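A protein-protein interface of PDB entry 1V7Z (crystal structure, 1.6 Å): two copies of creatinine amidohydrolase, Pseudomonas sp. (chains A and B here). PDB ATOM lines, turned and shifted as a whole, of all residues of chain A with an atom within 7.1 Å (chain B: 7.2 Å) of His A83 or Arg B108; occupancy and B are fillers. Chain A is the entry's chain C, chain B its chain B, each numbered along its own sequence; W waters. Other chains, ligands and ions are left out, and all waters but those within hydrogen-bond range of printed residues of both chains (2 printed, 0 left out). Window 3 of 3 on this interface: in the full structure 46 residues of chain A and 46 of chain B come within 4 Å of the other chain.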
ATOM      1  N   SER A  74      -9.272  16.205  19.484  1.00  0.00           N
ATOM      2  CA  SER A  74     -10.460  16.952  19.131  1.00  0.00           C
ATOM      3  C   SER A  74     -10.830  16.649  17.677  1.00  0.00           C
ATOM      4  O   SER A  74      -9.970  16.649  16.799  1.00  0.00           O
ATOM      5  CB  SER A  74     -10.193  18.450  19.326  1.00  0.00           C
ATOM      6  OG  SER A  74     -11.362  19.211  19.100  1.00  0.00           O
ATOM      7  N   GLN A  76     -13.378  17.598  14.331  1.00  0.00           N
ATOM      8  CA  GLN A  76     -14.012  18.793  13.780  1.00  0.00           C
ATOM      9  C   GLN A  76     -15.484  18.933  14.170  1.00  0.00           C
ATOM     10  O   GLN A  76     -15.912  20.000  14.616  1.00  0.00           O
ATOM     11  CB  GLN A  76     -13.885  18.795  12.257  1.00  0.00           C
ATOM     12  CG  GLN A  76     -14.490  20.020  11.602  1.00  0.00           C
ATOM     13  CD  GLN A  76     -13.859  20.326  10.266  1.00  0.00           C
ATOM     14  OE1 GLN A  76     -14.005  19.553   9.316  1.00  0.00           O
ATOM     15  NE2 GLN A  76     -13.150  21.444  10.187  1.00  0.00           N
ATOM     16  N   GLY A  79     -15.579  19.072  18.432  1.00  0.00           N
ATOM     17  CA  GLY A  79     -14.698  19.939  19.198  1.00  0.00           C
ATOM     18  C   GLY A  79     -13.926  20.967  18.400  1.00  0.00           C
ATOM     19  O   GLY A  79     -13.057  21.633  18.950  1.00  0.00           O
ATOM     20  N   GLY A  80     -14.234  21.100  17.111  1.00  0.00           N
ATOM     21  CA  GLY A  80     -13.572  22.070  16.256  1.00  0.00           C
ATOM     22  C   GLY A  80     -12.366  21.543  15.492  1.00  0.00           C
ATOM     23  O   GLY A  80     -12.070  22.021  14.400  1.00  0.00           O
ATOM     24  N   GLY A  81     -11.651  20.581  16.070  1.00  0.00           N
ATOM     25  CA  GLY A  81     -10.536  19.934  15.399  1.00  0.00           C
ATOM     26  C   GLY A  81      -9.228  20.095  16.151  1.00  0.00           C
ATOM     27  O   GLY A  81      -9.020  21.084  16.852  1.00  0.00           O
ATOM     28  N   ASN A  82      -8.328  19.138  15.965  1.00  0.00           N
ATOM     29  CA  ASN A  82      -7.062  19.113  16.703  1.00  0.00           C
ATOM     30  C   ASN A  82      -5.975  20.019  16.125  1.00  0.00           C
ATOM     31  O   ASN A  82      -4.837  20.014  16.594  1.00  0.00           O
ATOM     32  CB  ASN A  82      -6.534  17.681  16.807  1.00  0.00           C
ATOM     33  CG  ASN A  82      -5.754  17.452  18.076  1.00  0.00           C
ATOM     34  OD1 ASN A  82      -4.526  17.306  18.060  1.00  0.00           O
ATOM     35  ND2 ASN A  82      -6.455  17.467  19.185  1.00  0.00           N
ATOM     36  N   HIS A  83      -6.319  20.795  15.105  1.00  0.00           N
ATOM     37  CA  HIS A  83      -5.378  21.730  14.495  1.00  0.00           C
ATOM     38  C   HIS A  83      -5.269  23.057  15.267  1.00  0.00           C
ATOM     39  O   HIS A  83      -4.350  23.840  15.032  1.00  0.00           O
ATOM     40  CB  HIS A  83      -5.782  21.983  13.033  1.00  0.00           C
ATOM     41  CG  HIS A  83      -7.112  22.653  12.889  1.00  0.00           C
ATOM     42  ND1 HIS A  83      -8.275  22.104  13.383  1.00  0.00           N
ATOM     43  CD2 HIS A  83      -7.462  23.834  12.330  1.00  0.00           C
ATOM     44  CE1 HIS A  83      -9.283  22.923  13.138  1.00  0.00           C
ATOM     45  NE2 HIS A  83      -8.818  23.977  12.499  1.00  0.00           N
ATOM     46  N   PHE A  84      -6.189  23.306  16.196  1.00  0.00           N
ATOM     47  CA  PHE A  84      -6.142  24.529  16.999  1.00  0.00           C
ATOM     48  C   PHE A  84      -4.961  24.551  17.962  1.00  0.00           C
ATOM     49  O   PHE A  84      -4.571  23.505  18.491  1.00  0.00           O
ATOM     50  CB  PHE A  84      -7.427  24.706  17.813  1.00  0.00           C
ATOM     51  CG  PHE A  84      -8.559  25.299  17.026  1.00  0.00           C
ATOM     52  CD1 PHE A  84      -9.387  24.491  16.273  1.00  0.00           C
ATOM     53  CD2 PHE A  84      -8.797  26.668  17.048  1.00  0.00           C
ATOM     54  CE1 PHE A  84     -10.433  25.033  15.540  1.00  0.00           C
ATOM     55  CE2 PHE A  84      -9.841  27.217  16.313  1.00  0.00           C
ATOM     56  CZ  PHE A  84     -10.653  26.406  15.563  1.00  0.00           C
ATOM     57  N   PRO A  85      -4.421  25.741  18.223  1.00  0.00           N
ATOM     58  CA  PRO A  85      -3.458  25.926  19.311  1.00  0.00           C
ATOM     59  C   PRO A  85      -4.125  25.631  20.645  1.00  0.00           C
ATOM     60  O   PRO A  85      -5.350  25.746  20.747  1.00  0.00           O
ATOM     61  CB  PRO A  85      -3.103  27.422  19.236  1.00  0.00           C
ATOM     62  CG  PRO A  85      -3.678  27.930  17.981  1.00  0.00           C
ATOM     63  CD  PRO A  85      -4.737  27.007  17.540  1.00  0.00           C
ATOM     64  N   GLY A  86      -3.334  25.256  21.646  1.00  0.00           N
ATOM     65  CA  GLY A  86      -3.828  25.086  23.003  1.00  0.00           C
ATOM     66  C   GLY A  86      -4.359  23.690  23.271  1.00  0.00           C
ATOM     67  O   GLY A  86      -4.013  23.068  24.268  1.00  0.00           O
ATOM     68  N   THR A  87      -5.226  23.209  22.389  1.00  0.00           N
ATOM     69  CA  THR A  87      -5.710  21.836  22.449  1.00  0.00           C
ATOM     70  C   THR A  87      -4.519  20.895  22.513  1.00  0.00           C
ATOM     71  O   THR A  87      -3.653  20.930  21.647  1.00  0.00           O
ATOM     72  CB  THR A  87      -6.553  21.524  21.202  1.00  0.00           C
ATOM     73  OG1 THR A  87      -7.717  22.361  21.183  1.00  0.00           O
ATOM     74  CG2 THR A  87      -7.101  20.107  21.253  1.00  0.00           C
ATOM     75  N   THR A  88      -4.465  20.073  23.555  1.00  0.00           N
ATOM     76  CA  THR A  88      -3.323  19.202  23.807  1.00  0.00           C
ATOM     77  C   THR A  88      -3.847  17.799  24.042  1.00  0.00           C
ATOM     78  O   THR A  88      -4.371  17.495  25.114  1.00  0.00           O
ATOM     79  CB  THR A  88      -2.548  19.687  25.048  1.00  0.00           C
ATOM     80  OG1 THR A  88      -2.111  21.039  24.854  1.00  0.00           O
ATOM     81  CG2 THR A  88      -1.267  18.888  25.234  1.00  0.00           C
ATOM     82  N   SER A  89      -3.688  16.947  23.036  1.00  0.00           N
ATOM     83  CA  SER A  89      -4.391  15.670  22.975  1.00  0.00           C
ATOM     84  C   SER A  89      -3.499  14.437  23.040  1.00  0.00           C
ATOM     85  O   SER A  89      -2.391  14.418  22.522  1.00  0.00           O
ATOM     86  CB  SER A  89      -5.187  15.607  21.675  1.00  0.00           C
ATOM     87  OG  SER A  89      -6.123  16.660  21.634  1.00  0.00           O
ATOM     88  N   VAL A 216      -7.744  17.685   8.445  1.00  0.00           N
ATOM     89  CA  VAL A 216      -8.875  18.581   8.658  1.00  0.00           C
ATOM     90  C   VAL A 216      -8.707  19.862   7.858  1.00  0.00           C
ATOM     91  O   VAL A 216      -7.617  20.445   7.829  1.00  0.00           O
ATOM     92  CB  VAL A 216      -9.091  18.929  10.163  1.00  0.00           C
ATOM     93  CG1 VAL A 216      -7.895  19.669  10.753  1.00  0.00           C
ATOM     94  CG2 VAL A 216     -10.368  19.754  10.340  1.00  0.00           C
ATOM     95  N   ASP A 217      -9.783  20.260   7.184  1.00  0.00           N
ATOM     96  CA  ASP A 217      -9.879  21.553   6.523  1.00  0.00           C
ATOM     97  C   ASP A 217     -10.396  22.569   7.546  1.00  0.00           C
ATOM     98  O   ASP A 217     -11.573  22.521   7.921  1.00  0.00           O
ATOM     99  CB  ASP A 217     -10.834  21.468   5.335  1.00  0.00           C
ATOM    100  CG  ASP A 217     -11.102  22.820   4.701  1.00  0.00           C
ATOM    101  OD1 ASP A 217     -12.168  22.988   4.071  1.00  0.00           O
ATOM    102  OD2 ASP A 217     -10.308  23.777   4.788  1.00  0.00           O
ATOM    103  N   PRO A 218      -9.534  23.484   7.993  1.00  0.00           N
ATOM    104  CA  PRO A 218      -9.902  24.442   9.044  1.00  0.00           C
ATOM    105  C   PRO A 218     -11.069  25.374   8.690  1.00  0.00           C
ATOM    106  O   PRO A 218     -11.696  25.900   9.605  1.00  0.00           O
ATOM    107  CB  PRO A 218      -8.621  25.264   9.240  1.00  0.00           C
ATOM    108  CG  PRO A 218      -7.534  24.448   8.660  1.00  0.00           C
ATOM    109  CD  PRO A 218      -8.145  23.690   7.536  1.00  0.00           C
ATOM    110  N   ALA A 219     -11.339  25.580   7.400  1.00  0.00           N
ATOM    111  CA  ALA A 219     -12.438  26.448   6.971  1.00  0.00           C
ATOM    112  C   ALA A 219     -13.818  25.900   7.350  1.00  0.00           C
ATOM    113  O   ALA A 219     -14.771  26.668   7.499  1.00  0.00           O
ATOM    114  CB  ALA A 219     -12.361  26.693   5.463  1.00  0.00           C
ATOM    115  N   THR A 221     -14.605  24.583  10.198  1.00  0.00           N
ATOM    116  CA  THR A 221     -14.891  24.982  11.574  1.00  0.00           C
ATOM    117  C   THR A 221     -15.084  26.495  11.628  1.00  0.00           C
ATOM    118  O   THR A 221     -14.296  27.227  11.024  1.00  0.00           O
ATOM    119  CB  THR A 221     -13.709  24.593  12.496  1.00  0.00           C
ATOM    120  OG1 THR A 221     -13.507  23.178  12.458  1.00  0.00           O
ATOM    121  CG2 THR A 221     -14.021  24.883  13.966  1.00  0.00           C
ATOM    122  N   ILE B 102       2.184  14.840  25.003  1.00  0.00           N
ATOM    123  CA  ILE B 102       2.094  16.250  25.357  1.00  0.00           C
ATOM    124  C   ILE B 102       3.182  17.050  24.641  1.00  0.00           C
ATOM    125  O   ILE B 102       2.897  18.102  24.087  1.00  0.00           O
ATOM    126  CB  ILE B 102       2.129  16.464  26.899  1.00  0.00           C
ATOM    127  CG1 ILE B 102       0.824  15.944  27.509  1.00  0.00           C
ATOM    128  CG2 ILE B 102       2.298  17.937  27.224  1.00  0.00           C
ATOM    129  CD1 ILE B 102       0.872  15.721  29.009  1.00  0.00           C
ATOM    130  N   ILE B 103       4.414  16.548  24.624  1.00  0.00           N
ATOM    131  CA  ILE B 103       5.494  17.258  23.932  1.00  0.00           C
ATOM    132  C   ILE B 103       5.182  17.386  22.448  1.00  0.00           C
ATOM    133  O   ILE B 103       5.365  18.459  21.874  1.00  0.00           O
ATOM    134  CB  ILE B 103       6.853  16.580  24.149  1.00  0.00           C
ATOM    135  CG1 ILE B 103       7.257  16.725  25.620  1.00  0.00           C
ATOM    136  CG2 ILE B 103       7.923  17.195  23.228  1.00  0.00           C
ATOM    137  CD1 ILE B 103       8.429  15.881  26.020  1.00  0.00           C
ATOM    138  N   ARG B 104       4.706  16.308  21.830  1.00  0.00           N
ATOM    139  CA  ARG B 104       4.325  16.348  20.409  1.00  0.00           C
ATOM    140  C   ARG B 104       3.351  17.492  20.152  1.00  0.00           C
ATOM    141  O   ARG B 104       3.515  18.266  19.209  1.00  0.00           O
ATOM    142  CB  ARG B 104       3.677  15.027  19.988  1.00  0.00           C
ATOM    143  CG  ARG B 104       3.066  15.014  18.580  1.00  0.00           C
ATOM    144  CD  ARG B 104       2.277  13.746  18.250  1.00  0.00           C
ATOM    145  NE  ARG B 104       3.082  12.564  18.539  1.00  0.00           N
ATOM    146  CZ  ARG B 104       2.791  11.628  19.451  1.00  0.00           C
ATOM    147  NH1 ARG B 104       3.639  10.636  19.643  1.00  0.00           N
ATOM    148  NH2 ARG B 104       1.671  11.673  20.156  1.00  0.00           N
ATOM    149  N   GLU B 105       2.341  17.604  21.003  1.00  0.00           N
ATOM    150  CA  GLU B 105       1.303  18.620  20.835  1.00  0.00           C
ATOM    151  C   GLU B 105       1.804  20.035  21.100  1.00  0.00           C
ATOM    152  O   GLU B 105       1.461  20.964  20.367  1.00  0.00           O
ATOM    153  CB  GLU B 105       0.120  18.297  21.734  1.00  0.00           C
ATOM    154  CG  GLU B 105      -0.641  17.068  21.267  1.00  0.00           C
ATOM    155  CD  GLU B 105      -1.588  17.392  20.134  1.00  0.00           C
ATOM    156  OE1 GLU B 105      -2.741  17.773  20.424  1.00  0.00           O
ATOM    157  OE2 GLU B 105      -1.167  17.305  18.957  1.00  0.00           O
ATOM    158  N   LEU B 106       2.621  20.213  22.133  1.00  0.00           N
ATOM    159  CA  LEU B 106       3.208  21.522  22.399  1.00  0.00           C
ATOM    160  C   LEU B 106       4.077  21.974  21.228  1.00  0.00           C
ATOM    161  O   LEU B 106       4.058  23.149  20.844  1.00  0.00           O
ATOM    162  CB  LEU B 106       4.042  21.507  23.677  1.00  0.00           C
ATOM    163  CG  LEU B 106       3.227  21.326  24.959  1.00  0.00           C
ATOM    164  CD1 LEU B 106       4.160  21.311  26.157  1.00  0.00           C
ATOM    165  CD2 LEU B 106       2.144  22.403  25.119  1.00  0.00           C
ATOM    166  N   ALA B 107       4.823  21.040  20.652  1.00  0.00           N
ATOM    167  CA  ALA B 107       5.643  21.351  19.481  1.00  0.00           C
ATOM    168  C   ALA B 107       4.761  21.763  18.305  1.00  0.00           C
ATOM    169  O   ALA B 107       5.092  22.701  17.568  1.00  0.00           O
ATOM    170  CB  ALA B 107       6.510  20.183  19.112  1.00  0.00           C
ATOM    171  N   ARG B 108       3.629  21.086  18.146  1.00  0.00           N
ATOM    172  CA  ARG B 108       2.666  21.432  17.098  1.00  0.00           C
ATOM    173  C   ARG B 108       2.174  22.875  17.250  1.00  0.00           C
ATOM    174  O   ARG B 108       2.007  23.585  16.245  1.00  0.00           O
ATOM    175  CB  ARG B 108       1.480  20.454  17.096  1.00  0.00           C
ATOM    176  CG  ARG B 108       0.401  20.774  16.071  1.00  0.00           C
ATOM    177  CD  ARG B 108      -0.757  19.793  16.058  1.00  0.00           C
ATOM    178  NE  ARG B 108      -1.466  19.728  17.337  1.00  0.00           N
ATOM    179  CZ  ARG B 108      -2.262  20.683  17.814  1.00  0.00           C
ATOM    180  NH1 ARG B 108      -2.450  21.817  17.144  1.00  0.00           N
ATOM    181  NH2 ARG B 108      -2.869  20.513  18.985  1.00  0.00           N
ATOM    182  N   HIS B 109       1.938  23.308  18.489  1.00  0.00           N
ATOM    183  CA  HIS B 109       1.500  24.686  18.751  1.00  0.00           C
ATOM    184  C   HIS B 109       2.552  25.715  18.355  1.00  0.00           C
ATOM    185  O   HIS B 109       2.230  26.893  18.201  1.00  0.00           O
ATOM    186  CB  HIS B 109       1.190  24.935  20.230  1.00  0.00           C
ATOM    187  CG  HIS B 109       0.188  23.997  20.822  1.00  0.00           C
ATOM    188  ND1 HIS B 109       0.179  23.697  22.164  1.00  0.00           N
ATOM    189  CD2 HIS B 109      -0.823  23.288  20.269  1.00  0.00           C
ATOM    190  CE1 HIS B 109      -0.794  22.844  22.417  1.00  0.00           C
ATOM    191  NE2 HIS B 109      -1.415  22.572  21.284  1.00  0.00           N
ATOM    192  N   GLY B 110       3.806  25.279  18.254  1.00  0.00           N
ATOM    193  CA  GLY B 110       4.935  26.162  18.016  1.00  0.00           C
ATOM    194  C   GLY B 110       5.752  26.446  19.260  1.00  0.00           C
ATOM    195  O   GLY B 110       6.695  27.232  19.207  1.00  0.00           O
ATOM    196  N   ALA B 111       5.404  25.815  20.381  1.00  0.00           N
ATOM    197  CA  ALA B 111       6.195  25.931  21.604  1.00  0.00           C
ATOM    198  C   ALA B 111       7.532  25.221  21.418  1.00  0.00           C
ATOM    199  O   ALA B 111       7.620  24.241  20.688  1.00  0.00           O
ATOM    200  CB  ALA B 111       5.448  25.341  22.781  1.00  0.00           C
ATOM    201  N   ARG B 112       8.572  25.724  22.073  1.00  0.00           N
ATOM    202  CA  ARG B 112       9.913  25.155  21.948  1.00  0.00           C
ATOM    203  C   ARG B 112      10.698  25.100  23.267  1.00  0.00           C
ATOM    204  O   ARG B 112      11.876  24.749  23.268  1.00  0.00           O
ATOM    205  CB  ARG B 112      10.709  25.953  20.904  1.00  0.00           C
ATOM    206  CG  ARG B 112      10.232  25.756  19.472  1.00  0.00           C
ATOM    207  CD  ARG B 112      10.525  24.376  18.923  1.00  0.00           C
ATOM    208  NE  ARG B 112      10.210  24.208  17.504  1.00  0.00           N
ATOM    209  CZ  ARG B 112       9.025  23.843  17.026  1.00  0.00           C
ATOM    210  NH1 ARG B 112       7.994  23.623  17.831  1.00  0.00           N
ATOM    211  NH2 ARG B 112       8.866  23.692  15.718  1.00  0.00           N
ATOM    212  N   LEU B 138      10.446  14.577  16.628  1.00  0.00           N
ATOM    213  CA  LEU B 138      10.699  15.940  16.151  1.00  0.00           C
ATOM    214  C   LEU B 138      11.895  15.956  15.187  1.00  0.00           C
ATOM    215  O   LEU B 138      11.856  16.654  14.169  1.00  0.00           O
ATOM    216  CB  LEU B 138      10.899  16.905  17.323  1.00  0.00           C
ATOM    217  CG  LEU B 138       9.613  17.213  18.099  1.00  0.00           C
ATOM    218  CD1 LEU B 138       9.911  17.975  19.378  1.00  0.00           C
ATOM    219  CD2 LEU B 138       8.599  17.961  17.243  1.00  0.00           C
ATOM    220  N   ILE B 143      13.406  19.080  13.248  1.00  0.00           N
ATOM    221  CA  ILE B 143      13.307  19.996  14.383  1.00  0.00           C
ATOM    222  C   ILE B 143      14.264  19.598  15.496  1.00  0.00           C
ATOM    223  O   ILE B 143      14.165  18.486  16.033  1.00  0.00           O
ATOM    224  CB  ILE B 143      11.859  20.010  14.919  1.00  0.00           C
ATOM    225  CG1 ILE B 143      10.909  20.583  13.863  1.00  0.00           C
ATOM    226  CG2 ILE B 143      11.766  20.803  16.215  1.00  0.00           C
ATOM    227  CD1 ILE B 143       9.439  20.321  14.149  1.00  0.00           C
ATOM    228  N   PHE B 146      13.490  22.301  19.979  1.00  0.00           N
ATOM    229  CA  PHE B 146      12.662  22.060  21.165  1.00  0.00           C
ATOM    230  C   PHE B 146      13.584  21.624  22.293  1.00  0.00           C
ATOM    231  O   PHE B 146      14.258  20.613  22.177  1.00  0.00           O
ATOM    232  CB  PHE B 146      11.602  20.982  20.910  1.00  0.00           C
ATOM    233  CG  PHE B 146      10.453  21.021  21.883  1.00  0.00           C
ATOM    234  CD1 PHE B 146      10.611  20.558  23.177  1.00  0.00           C
ATOM    235  CD2 PHE B 146       9.215  21.518  21.506  1.00  0.00           C
ATOM    236  CE1 PHE B 146       9.555  20.597  24.072  1.00  0.00           C
ATOM    237  CE2 PHE B 146       8.163  21.565  22.396  1.00  0.00           C
ATOM    238  CZ  PHE B 146       8.335  21.101  23.686  1.00  0.00           C
HETATM  239  O   HOH W   1      -1.101  12.897  20.496  1.00  0.00           O
HETATM  240  O   HOH W   2      -1.895  22.787  14.460  1.00  0.00           O
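No position is printed for both chains. Of the 12 pairs that touch across the chains among the printed residues, none has its exchanged pair printed and touching as well.
Of the printed residues of chain B, His A83 touches Arg B108. Printed residues of chain B within 4 Å of Phe A84: Arg B108 (3.0 Å). Of the printed residues of chain B, Pro A85 touches His B109 (3.8 Å). Printed residues of chain B within 4 Å of Gly A86: His B109 (3.3 Å). Of the printed residues of chain B, Thr A88 touches Glu B105 (3.7 Å) and His B109 (3.3 Å). Printed residues of chain A within 4 Å of Glu B105: Asn A82, Thr A87, Thr A88 and Ser A89. Printed residues of chain A within 4 Å of Arg B108: Asn A82, His A83, Phe A84 and Thr A87. The nearest residue of chain B that does not touch His A83 is His B109 (6.3 Å). The nearest residue of chain A that does not touch Arg B108 is Pro A85 (4.5 Å). The nearest printed residue of chain B that does not touch Ser A89 is Ile B102 (5.2 Å).
Water W2 lies within hydrogen-bond range of the backbone carbonyl oxygen of His A83 (2.7 Å) and the guanidinium group of Arg B108 (2.9 Å). Water W1 lies within hydrogen-bond range of the backbone carbonyl oxygen of Ser A89 and the guanidinium group of Arg B104.
Of the 14 printed residues of chain B, 3 touch a printed residue of chain A. Printed residues of chain B that touch a printed residue of chain A: Glu B105, Arg B108 and His B109. Hydrophobic or aromatic side chains of chain B that line the printed part of chain A: His B109. Of the 18 printed residues of chain A, 8 touch a printed residue of chain B. Among the printed residues, no Asp or Glu carboxylate lies within 4 Å of a Lys or Arg side-chain nitrogen of the other chain.
NH2 of Arg B108 lies within hydrogen-bond range of O of Thr A87, at 2.8 Å. The side-chain carboxylate of Glu B105 lies close to the side-chain amide oxygen of Asn A82. The guanidinium group (NH1) of Arg B108 lies close to the backbone carbonyl oxygen (O) of Asn A82 (3.0 Å). The backbone carbonyl oxygen of His A83 lies within hydrogen-bond range of the guanidinium group of Arg B108 (3.5 Å). A ring nitrogen (NE2) of His B109 is in hydrogen-bond range of the backbone carbonyl oxygen (O) of Thr A87, at 2.8 Å. NE2 of His B109 sits at hydrogen-bond distance from N of Gly A86 (3.3 Å). The side-chain carboxylate of Glu B105 is in hydrogen-bond range of the backbone NH of Ser A89 (2.9 Å). NH1 of Arg B108 is in hydrogen-bond range of O of Phe A84.
CA of Pro A85 touches CD2 of His B109, at 3.8 Å. Thr A87 touches Glu B105 (O to OE1, 3.5 Å). CA of Thr A88 touches OE1 of Glu B105 (3.7 Å). Thr A88 touches His B109 (OG1 to CE1, 3.3 Å).
The guanidinium group (NH2) of Arg B108 sits at hydrogen-bond distance from a ring nitrogen (NE2) of His B109, 3.4 Å away. The backbone carbonyl oxygen (O) of Gly A86 sits at hydrogen-bond distance from the side-chain hydroxyl (OG1) of Thr A88, 2.8 Å away. The backbone carbonyl oxygen (O) of Ser A74 is in hydrogen-bond range of the backbone NH (N) of Asn A82, at 3.1 Å. The backbone carbonyl oxygen (O) of Glu B105 sits close to a ring nitrogen (NE2) of His B109, 3.4 Å away. OG of Ser A89 is in hydrogen-bond range of ND2 of Asn A82 (2.6 Å). NE of Arg B108 is in salt-bridge range of OE2 of Glu B105 (2.9 Å).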
